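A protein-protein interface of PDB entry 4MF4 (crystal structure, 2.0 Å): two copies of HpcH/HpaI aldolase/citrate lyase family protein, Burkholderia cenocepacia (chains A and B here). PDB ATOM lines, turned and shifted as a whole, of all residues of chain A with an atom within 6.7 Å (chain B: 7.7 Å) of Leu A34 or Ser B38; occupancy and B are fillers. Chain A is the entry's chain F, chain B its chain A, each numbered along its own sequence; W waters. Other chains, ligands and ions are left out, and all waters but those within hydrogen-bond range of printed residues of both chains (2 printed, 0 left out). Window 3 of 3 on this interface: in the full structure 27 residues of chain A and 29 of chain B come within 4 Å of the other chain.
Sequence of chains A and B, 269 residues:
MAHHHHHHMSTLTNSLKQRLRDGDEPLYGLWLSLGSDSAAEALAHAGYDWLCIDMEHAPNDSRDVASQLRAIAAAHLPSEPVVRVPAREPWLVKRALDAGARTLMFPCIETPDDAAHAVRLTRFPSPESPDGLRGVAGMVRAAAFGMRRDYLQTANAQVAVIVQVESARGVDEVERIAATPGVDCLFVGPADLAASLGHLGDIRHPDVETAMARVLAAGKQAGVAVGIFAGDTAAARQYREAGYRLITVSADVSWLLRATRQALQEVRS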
ATOM      1  N   TRP A  31      27.390 -20.353  27.930  1.00  0.00           N
ATOM      2  CA  TRP A  31      27.536 -19.013  27.389  1.00  0.00           C
ATOM      3  C   TRP A  31      26.176 -18.407  27.206  1.00  0.00           C
ATOM      4  O   TRP A  31      25.269 -19.059  26.614  1.00  0.00           O
ATOM      5  CB  TRP A  31      28.276 -19.067  26.022  1.00  0.00           C
ATOM      6  CG  TRP A  31      29.174 -17.867  25.713  1.00  0.00           C
ATOM      7  CD1 TRP A  31      28.900 -16.816  24.879  1.00  0.00           C
ATOM      8  CD2 TRP A  31      30.506 -17.659  26.199  1.00  0.00           C
ATOM      9  NE1 TRP A  31      29.968 -15.954  24.852  1.00  0.00           N
ATOM     10  CE2 TRP A  31      30.963 -16.442  25.659  1.00  0.00           C
ATOM     11  CE3 TRP A  31      31.358 -18.390  27.039  1.00  0.00           C
ATOM     12  CZ2 TRP A  31      32.242 -15.920  25.945  1.00  0.00           C
ATOM     13  CZ3 TRP A  31      32.623 -17.869  27.325  1.00  0.00           C
ATOM     14  CH2 TRP A  31      33.059 -16.645  26.746  1.00  0.00           C
ATOM     15  N   LEU A  32      26.010 -17.177  27.729  1.00  0.00           N
ATOM     16  CA  LEU A  32      24.756 -16.401  27.595  1.00  0.00           C
ATOM     17  C   LEU A  32      24.961 -15.298  26.572  1.00  0.00           C
ATOM     18  O   LEU A  32      25.568 -14.246  26.870  1.00  0.00           O
ATOM     19  CB  LEU A  32      24.295 -15.773  28.934  1.00  0.00           C
ATOM     20  CG  LEU A  32      24.256 -16.644  30.198  1.00  0.00           C
ATOM     21  CD1 LEU A  32      23.748 -15.909  31.432  1.00  0.00           C
ATOM     22  CD2 LEU A  32      23.471 -17.934  30.026  1.00  0.00           C
ATOM     23  N   SER A  33      24.460 -15.568  25.365  1.00  0.00           N
ATOM     24  CA  SER A  33      24.529 -14.692  24.199  1.00  0.00           C
ATOM     25  C   SER A  33      23.231 -13.927  23.895  1.00  0.00           C
ATOM     26  O   SER A  33      23.236 -13.014  23.074  1.00  0.00           O
ATOM     27  CB  SER A  33      24.797 -15.528  22.937  1.00  0.00           C
ATOM     28  OG  SER A  33      26.133 -16.001  22.912  1.00  0.00           O
ATOM     29  N   LEU A  34      22.115 -14.349  24.476  1.00  0.00           N
ATOM     30  CA  LEU A  34      20.804 -13.818  24.078  1.00  0.00           C
ATOM     31  C   LEU A  34      20.488 -12.449  24.670  1.00  0.00           C
ATOM     32  O   LEU A  34      19.580 -11.772  24.202  1.00  0.00           O
ATOM     33  CB  LEU A  34      19.689 -14.785  24.465  1.00  0.00           C
ATOM     34  CG  LEU A  34      19.561 -16.069  23.652  1.00  0.00           C
ATOM     35  CD1 LEU A  34      18.784 -17.130  24.404  1.00  0.00           C
ATOM     36  CD2 LEU A  34      18.890 -15.775  22.336  1.00  0.00           C
ATOM     37  N   GLY A  35      21.197 -12.079  25.723  1.00  0.00           N
ATOM     38  CA  GLY A  35      20.944 -10.819  26.436  1.00  0.00           C
ATOM     39  C   GLY A  35      19.617 -10.754  27.184  1.00  0.00           C
ATOM     40  O   GLY A  35      19.107  -9.661  27.420  1.00  0.00           O
ATOM     41  N   SER A  36      19.090 -11.905  27.607  1.00  0.00           N
ATOM     42  CA  SER A  36      17.766 -12.006  28.190  1.00  0.00           C
ATOM     43  C   SER A  36      17.806 -12.306  29.708  1.00  0.00           C
ATOM     44  O   SER A  36      18.384 -13.310  30.123  1.00  0.00           O
ATOM     45  CB  SER A  36      16.990 -13.140  27.466  1.00  0.00           C
ATOM     46  OG  SER A  36      15.903 -13.630  28.234  1.00  0.00           O
ATOM     47  N   ALA A  39      16.051 -15.703  30.325  1.00  0.00           N
ATOM     48  CA  ALA A  39      16.920 -16.820  29.967  1.00  0.00           C
ATOM     49  C   ALA A  39      18.007 -17.031  31.003  1.00  0.00           C
ATOM     50  O   ALA A  39      18.314 -18.168  31.299  1.00  0.00           O
ATOM     51  CB  ALA A  39      17.557 -16.625  28.595  1.00  0.00           C
ATOM     52  N   LEU A  43      18.259 -20.399  33.250  1.00  0.00           N
ATOM     53  CA  LEU A  43      19.472 -21.150  33.128  1.00  0.00           C
ATOM     54  C   LEU A  43      20.246 -21.201  34.479  1.00  0.00           C
ATOM     55  O   LEU A  43      20.956 -22.177  34.735  1.00  0.00           O
ATOM     56  CB  LEU A  43      20.295 -20.639  31.931  1.00  0.00           C
ATOM     57  CG  LEU A  43      19.770 -20.981  30.526  1.00  0.00           C
ATOM     58  CD1 LEU A  43      20.688 -20.329  29.477  1.00  0.00           C
ATOM     59  CD2 LEU A  43      19.663 -22.475  30.274  1.00  0.00           C
ATOM     60  N   ALA A  58      28.252 -10.183  22.317  1.00  0.00           N
ATOM     61  CA  ALA A  58      26.831 -10.062  22.553  1.00  0.00           C
ATOM     62  C   ALA A  58      26.598  -8.620  23.027  1.00  0.00           C
ATOM     63  O   ALA A  58      27.522  -8.029  23.620  1.00  0.00           O
ATOM     64  CB  ALA A  58      26.376 -11.056  23.585  1.00  0.00           C
ATOM     65  N   PRO A  59      25.418  -8.023  22.699  1.00  0.00           N
ATOM     66  CA  PRO A  59      25.167  -6.593  22.939  1.00  0.00           C
ATOM     67  C   PRO A  59      24.722  -6.324  24.394  1.00  0.00           C
ATOM     68  O   PRO A  59      23.586  -5.898  24.642  1.00  0.00           O
ATOM     69  CB  PRO A  59      24.050  -6.264  21.923  1.00  0.00           C
ATOM     70  CG  PRO A  59      23.247  -7.542  21.805  1.00  0.00           C
ATOM     71  CD  PRO A  59      24.253  -8.683  22.063  1.00  0.00           C
ATOM     72  N   ASN A  60      25.609  -6.619  25.346  1.00  0.00           N
ATOM     73  CA  ASN A  60      25.329  -6.445  26.755  1.00  0.00           C
ATOM     74  C   ASN A  60      26.131  -5.283  27.261  1.00  0.00           C
ATOM     75  O   ASN A  60      27.362  -5.352  27.343  1.00  0.00           O
ATOM     76  CB  ASN A  60      25.694  -7.726  27.540  1.00  0.00           C
ATOM     77  CG  ASN A  60      24.691  -8.835  27.310  1.00  0.00           C
ATOM     78  OD1 ASN A  60      23.492  -8.589  27.358  1.00  0.00           O
ATOM     79  ND2 ASN A  60      25.172 -10.052  27.081  1.00  0.00           N
ATOM     80  N   GLN A  68      21.229  -9.038  34.351  1.00  0.00           N
ATOM     81  CA  GLN A  68      21.448 -10.501  34.280  1.00  0.00           C
ATOM     82  C   GLN A  68      22.086 -11.036  35.544  1.00  0.00           C
ATOM     83  O   GLN A  68      21.789 -12.174  35.951  1.00  0.00           O
ATOM     84  CB  GLN A  68      22.232 -10.859  33.028  1.00  0.00           C
ATOM     85  CG  GLN A  68      21.337 -10.832  31.791  1.00  0.00           C
ATOM     86  CD  GLN A  68      22.115 -10.760  30.503  1.00  0.00           C
ATOM     87  OE1 GLN A  68      22.691 -11.743  30.065  1.00  0.00           O
ATOM     88  NE2 GLN A  68      22.141  -9.592  29.892  1.00  0.00           N
ATOM     89  N   ASP A 252      23.639 -20.662  25.089  1.00  0.00           N
ATOM     90  CA  ASP A 252      22.185 -20.676  25.196  1.00  0.00           C
ATOM     91  C   ASP A 252      21.503 -20.764  23.835  1.00  0.00           C
ATOM     92  O   ASP A 252      20.622 -21.583  23.652  1.00  0.00           O
ATOM     93  CB  ASP A 252      21.627 -19.470  25.980  1.00  0.00           C
ATOM     94  CG  ASP A 252      22.123 -18.113  25.464  1.00  0.00           C
ATOM     95  OD1 ASP A 252      22.857 -18.052  24.440  1.00  0.00           O
ATOM     96  OD2 ASP A 252      21.765 -17.084  26.091  1.00  0.00           O
ATOM     97  N   VAL A 253      21.863 -19.897  22.894  1.00  0.00           N
ATOM     98  CA  VAL A 253      21.083 -19.850  21.630  1.00  0.00           C
ATOM     99  C   VAL A 253      21.292 -21.104  20.792  1.00  0.00           C
ATOM    100  O   VAL A 253      20.380 -21.513  20.079  1.00  0.00           O
ATOM    101  CB  VAL A 253      21.318 -18.572  20.799  1.00  0.00           C
ATOM    102  CG1 VAL A 253      22.728 -18.496  20.224  1.00  0.00           C
ATOM    103  CG2 VAL A 253      20.256 -18.436  19.717  1.00  0.00           C
ATOM    104  N   LEU A 256      19.154 -23.803  22.211  1.00  0.00           N
ATOM    105  CA  LEU A 256      17.777 -23.484  21.924  1.00  0.00           C
ATOM    106  C   LEU A 256      17.408 -23.892  20.473  1.00  0.00           C
ATOM    107  O   LEU A 256      16.370 -24.475  20.234  1.00  0.00           O
ATOM    108  CB  LEU A 256      17.527 -21.991  22.141  1.00  0.00           C
ATOM    109  CG  LEU A 256      16.122 -21.539  21.773  1.00  0.00           C
ATOM    110  CD1 LEU A 256      15.074 -22.222  22.644  1.00  0.00           C
ATOM    111  CD2 LEU A 256      16.037 -20.032  21.853  1.00  0.00           C
ATOM    112  N   LEU B  34       9.933 -16.357  26.393  1.00  0.00           N
ATOM    113  CA  LEU B  34      11.117 -15.705  26.947  1.00  0.00           C
ATOM    114  C   LEU B  34      11.108 -14.183  26.787  1.00  0.00           C
ATOM    115  O   LEU B  34      11.829 -13.478  27.523  1.00  0.00           O
ATOM    116  CB  LEU B  34      12.415 -16.282  26.332  1.00  0.00           C
ATOM    117  CG  LEU B  34      12.854 -17.716  26.671  1.00  0.00           C
ATOM    118  CD1 LEU B  34      13.957 -18.134  25.678  1.00  0.00           C
ATOM    119  CD2 LEU B  34      13.314 -17.757  28.121  1.00  0.00           C
ATOM    120  N   GLY B  35      10.294 -13.654  25.886  1.00  0.00           N
ATOM    121  CA  GLY B  35      10.208 -12.201  25.723  1.00  0.00           C
ATOM    122  C   GLY B  35      11.417 -11.531  25.101  1.00  0.00           C
ATOM    123  O   GLY B  35      11.680 -10.344  25.338  1.00  0.00           O
ATOM    124  N   SER B  36      12.134 -12.284  24.277  1.00  0.00           N
ATOM    125  CA  SER B  36      13.458 -11.918  23.788  1.00  0.00           C
ATOM    126  C   SER B  36      13.421 -11.708  22.285  1.00  0.00           C
ATOM    127  O   SER B  36      13.011 -12.612  21.562  1.00  0.00           O
ATOM    128  CB  SER B  36      14.434 -13.098  24.101  1.00  0.00           C
ATOM    129  OG  SER B  36      15.688 -12.933  23.413  1.00  0.00           O
ATOM    130  N   ASP B  37      13.864 -10.549  21.809  1.00  0.00           N
ATOM    131  CA  ASP B  37      13.927 -10.284  20.338  1.00  0.00           C
ATOM    132  C   ASP B  37      14.922 -11.219  19.635  1.00  0.00           C
ATOM    133  O   ASP B  37      14.655 -11.768  18.581  1.00  0.00           O
ATOM    134  CB  ASP B  37      14.318  -8.824  20.029  1.00  0.00           C
ATOM    135  CG  ASP B  37      13.303  -7.817  20.503  1.00  0.00           C
ATOM    136  OD1 ASP B  37      12.134  -8.175  20.806  1.00  0.00           O
ATOM    137  OD2 ASP B  37      13.696  -6.634  20.558  1.00  0.00           O
ATOM    138  N   SER B  38      16.083 -11.405  20.253  1.00  0.00           N
ATOM    139  CA  SER B  38      17.100 -12.274  19.678  1.00  0.00           C
ATOM    140  C   SER B  38      16.602 -13.717  19.612  1.00  0.00           C
ATOM    141  O   SER B  38      16.817 -14.387  18.617  1.00  0.00           O
ATOM    142  CB  SER B  38      18.414 -12.153  20.465  1.00  0.00           C
ATOM    143  OG  SER B  38      18.174 -12.194  21.858  1.00  0.00           O
ATOM    144  N   ALA B  39      15.891 -14.167  20.645  1.00  0.00           N
ATOM    145  CA  ALA B  39      15.363 -15.531  20.677  1.00  0.00           C
ATOM    146  C   ALA B  39      14.320 -15.713  19.593  1.00  0.00           C
ATOM    147  O   ALA B  39      14.301 -16.755  18.935  1.00  0.00           O
ATOM    148  CB  ALA B  39      14.763 -15.904  22.022  1.00  0.00           C
ATOM    149  N   ALA B  40      13.479 -14.699  19.404  1.00  0.00           N
ATOM    150  CA  ALA B  40      12.411 -14.757  18.381  1.00  0.00           C
ATOM    151  C   ALA B  40      13.024 -14.796  16.980  1.00  0.00           C
ATOM    152  O   ALA B  40      12.548 -15.555  16.086  1.00  0.00           O
ATOM    153  CB  ALA B  40      11.484 -13.556  18.499  1.00  0.00           C
ATOM    154  N   GLU B  41      14.032 -13.963  16.771  1.00  0.00           N
ATOM    155  CA  GLU B  41      14.710 -13.926  15.481  1.00  0.00           C
ATOM    156  C   GLU B  41      15.445 -15.231  15.231  1.00  0.00           C
ATOM    157  O   GLU B  41      15.296 -15.840  14.149  1.00  0.00           O
ATOM    158  CB  GLU B  41      15.683 -12.756  15.333  1.00  0.00           C
ATOM    159  CG  GLU B  41      16.142 -12.634  13.890  1.00  0.00           C
ATOM    160  CD  GLU B  41      16.977 -11.433  13.574  1.00  0.00           C
ATOM    161  OE1 GLU B  41      17.311 -10.617  14.474  1.00  0.00           O
ATOM    162  OE2 GLU B  41      17.302 -11.309  12.356  1.00  0.00           O
ATOM    163  N   ALA B  42      16.171 -15.720  16.241  1.00  0.00           N
ATOM    164  CA  ALA B  42      16.787 -17.057  16.106  1.00  0.00           C
ATOM    165  C   ALA B  42      15.752 -18.149  15.763  1.00  0.00           C
ATOM    166  O   ALA B  42      15.922 -18.911  14.815  1.00  0.00           O
ATOM    167  CB  ALA B  42      17.595 -17.402  17.362  1.00  0.00           C
ATOM    168  N   LEU B  43      14.671 -18.237  16.538  1.00  0.00           N
ATOM    169  CA  LEU B  43      13.647 -19.259  16.303  1.00  0.00           C
ATOM    170  C   LEU B  43      12.892 -19.141  14.971  1.00  0.00           C
ATOM    171  O   LEU B  43      12.373 -20.133  14.452  1.00  0.00           O
ATOM    172  CB  LEU B  43      12.708 -19.374  17.525  1.00  0.00           C
ATOM    173  CG  LEU B  43      13.415 -19.909  18.754  1.00  0.00           C
ATOM    174  CD1 LEU B  43      12.535 -19.786  20.003  1.00  0.00           C
ATOM    175  CD2 LEU B  43      13.832 -21.375  18.555  1.00  0.00           C
ATOM    176  N   ALA B  44      12.842 -17.942  14.418  1.00  0.00           N
ATOM    177  CA  ALA B  44      12.372 -17.736  13.055  1.00  0.00           C
ATOM    178  C   ALA B  44      13.163 -18.515  11.992  1.00  0.00           C
ATOM    179  O   ALA B  44      12.661 -18.676  10.854  1.00  0.00           O
ATOM    180  CB  ALA B  44      12.312 -16.252  12.718  1.00  0.00           C
ATOM    181  N   HIS B  45      14.316 -19.084  12.384  1.00  0.00           N
ATOM    182  CA  HIS B  45      15.148 -19.926  11.527  1.00  0.00           C
ATOM    183  C   HIS B  45      14.967 -21.422  11.851  1.00  0.00           C
ATOM    184  O   HIS B  45      15.670 -22.267  11.325  1.00  0.00           O
ATOM    185  CB  HIS B  45      16.639 -19.577  11.696  1.00  0.00           C
ATOM    186  CG  HIS B  45      17.018 -18.237  11.167  1.00  0.00           C
ATOM    187  ND1 HIS B  45      17.606 -18.060   9.928  1.00  0.00           N
ATOM    188  CD2 HIS B  45      16.862 -16.999  11.686  1.00  0.00           C
ATOM    189  CE1 HIS B  45      17.839 -16.775   9.732  1.00  0.00           C
ATOM    190  NE2 HIS B  45      17.382 -16.111  10.773  1.00  0.00           N
ATOM    191  N   SER B  67       8.339  -5.445  18.810  1.00  0.00           N
ATOM    192  CA  SER B  67       9.758  -5.745  18.675  1.00  0.00           C
ATOM    193  C   SER B  67      10.027  -7.241  18.298  1.00  0.00           C
ATOM    194  O   SER B  67      10.963  -7.539  17.530  1.00  0.00           O
ATOM    195  CB  SER B  67      10.477  -5.338  19.961  1.00  0.00           C
ATOM    196  OG  SER B  67      10.374  -3.922  20.155  1.00  0.00           O
ATOM    197  N   GLN B  68       9.209  -8.150  18.825  1.00  0.00           N
ATOM    198  CA  GLN B  68       9.273  -9.577  18.443  1.00  0.00           C
ATOM    199  C   GLN B  68       8.711  -9.830  17.035  1.00  0.00           C
ATOM    200  O   GLN B  68       9.255 -10.644  16.258  1.00  0.00           O
ATOM    201  CB  GLN B  68       8.639 -10.478  19.461  1.00  0.00           C
ATOM    202  CG  GLN B  68       9.564 -10.637  20.633  1.00  0.00           C
ATOM    203  CD  GLN B  68       8.860 -11.214  21.830  1.00  0.00           C
ATOM    204  OE1 GLN B  68       8.614 -12.436  21.886  1.00  0.00           O
ATOM    205  NE2 GLN B  68       8.553 -10.360  22.803  1.00  0.00           N
ATOM    206  N   ALA B  71      11.376  -8.722  14.827  1.00  0.00           N
ATOM    207  CA  ALA B  71      12.520  -9.612  14.907  1.00  0.00           C
ATOM    208  C   ALA B  71      12.290 -10.895  14.067  1.00  0.00           C
ATOM    209  O   ALA B  71      13.173 -11.363  13.375  1.00  0.00           O
ATOM    210  CB  ALA B  71      12.823  -9.988  16.352  1.00  0.00           C
ATOM    211  N   LEU B 256      14.887 -24.916  25.992  1.00  0.00           N
ATOM    212  CA  LEU B 256      16.146 -24.379  26.467  1.00  0.00           C
ATOM    213  C   LEU B 256      16.645 -25.065  27.722  1.00  0.00           C
ATOM    214  O   LEU B 256      17.814 -25.453  27.804  1.00  0.00           O
ATOM    215  CB  LEU B 256      16.018 -22.858  26.723  1.00  0.00           C
ATOM    216  CG  LEU B 256      17.229 -22.150  27.297  1.00  0.00           C
ATOM    217  CD1 LEU B 256      18.435 -22.256  26.397  1.00  0.00           C
ATOM    218  CD2 LEU B 256      16.918 -20.696  27.550  1.00  0.00           C
HETATM  219  O   HOH W   1      13.792 -11.853  27.869  1.00  0.00           O
HETATM  220  O   HOH W   2      17.113 -10.846  24.355  1.00  0.00           O
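OG of Ser B38 lies within hydrogen-bond range of O of Leu A34, 2.8 Å away.
N of Leu A34 sits at hydrogen-bond distance from OD2 of Asp A252 (3.2 Å).
O of Trp A31 sits at hydrogen-bond distance from N of Asp A252 (2.7 Å).
The side-chain hydroxyl of Ser B38 is in hydrogen-bond range of the side-chain hydroxyl of Ser B36 (3.0 Å).
OG of Ser B36 lies within hydrogen-bond range of N of Ala B39, at 3.0 Å.
The backbone NH of Ser A33 sits at hydrogen-bond distance from the side-chain carboxylate of Asp A252 (3.1 Å).
Ala B39 touches Leu A34 (N to CD2, 3.8 Å).
Leu A43 touches Leu B256 (CD2 to CG, 3.9 Å).
Asp A252 touches Leu B256.
CB of Ala B42 touches CG2 of Val A253, at 3.7 Å.
CG of Leu A256 touches CD2 of Leu B43, 3.95 Å away.
Of the printed residues of chain B, Leu A34 touches Ser B38 and Ala B39.
Of the printed residues of chain A, Leu B43 touches Leu A256 (3.95 Å).
Of the printed residues of chain B, Val A253 touches Ala B42.
Of the printed residues of chain B, Asp A252 touches Leu B256.
Printed residues of chain B within 4 Å of Leu A256: Leu B43 (3.95 Å).
Ala B44 touches none of the printed residues of chain A.
The nearest printed residue of chain A that does not touch Ser B38 is Gly A35 (4.9 Å).
Printed residues of chain B that touch a printed residue of chain A: Ser B38, Ala B39, Ala B42, Leu B43 and Leu B256.
Of the 15 printed residues of chain A, 5 touch a printed residue of chain B.
Hydrophobic or aromatic side chains of chain A within 4 Å of the printed part of chain B: Leu A34, Leu A43, Val A253 and Leu A256.
Among the printed residues, 6 pairs touch across the chains.
Leu A34 touches Ala B39, but with the chains exchanged Ala A39 does not touch Leu B34 (4.1 Å).
Leu A43 touches Leu B256, and with the chains exchanged Leu A256 touches Leu B43.
7 positions are printed for both chains.
Of the 6 pairs that touch across the chains among the printed residues, 2 have their exchanged pair printed and touching as well.
Water W1 lies within hydrogen-bond range of O of Leu B34 (2.6 Å) and OG of Ser A36 (2.8 Å).
Water W2 lies within hydrogen-bond range of the backbone carbonyl oxygen (O) of Leu A34 (2.6 Å), the side-chain hydroxyl (OG) of Ser B36 (2.7 Å) and the side-chain hydroxyl (OG) of Ser B38 (3.0 Å).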
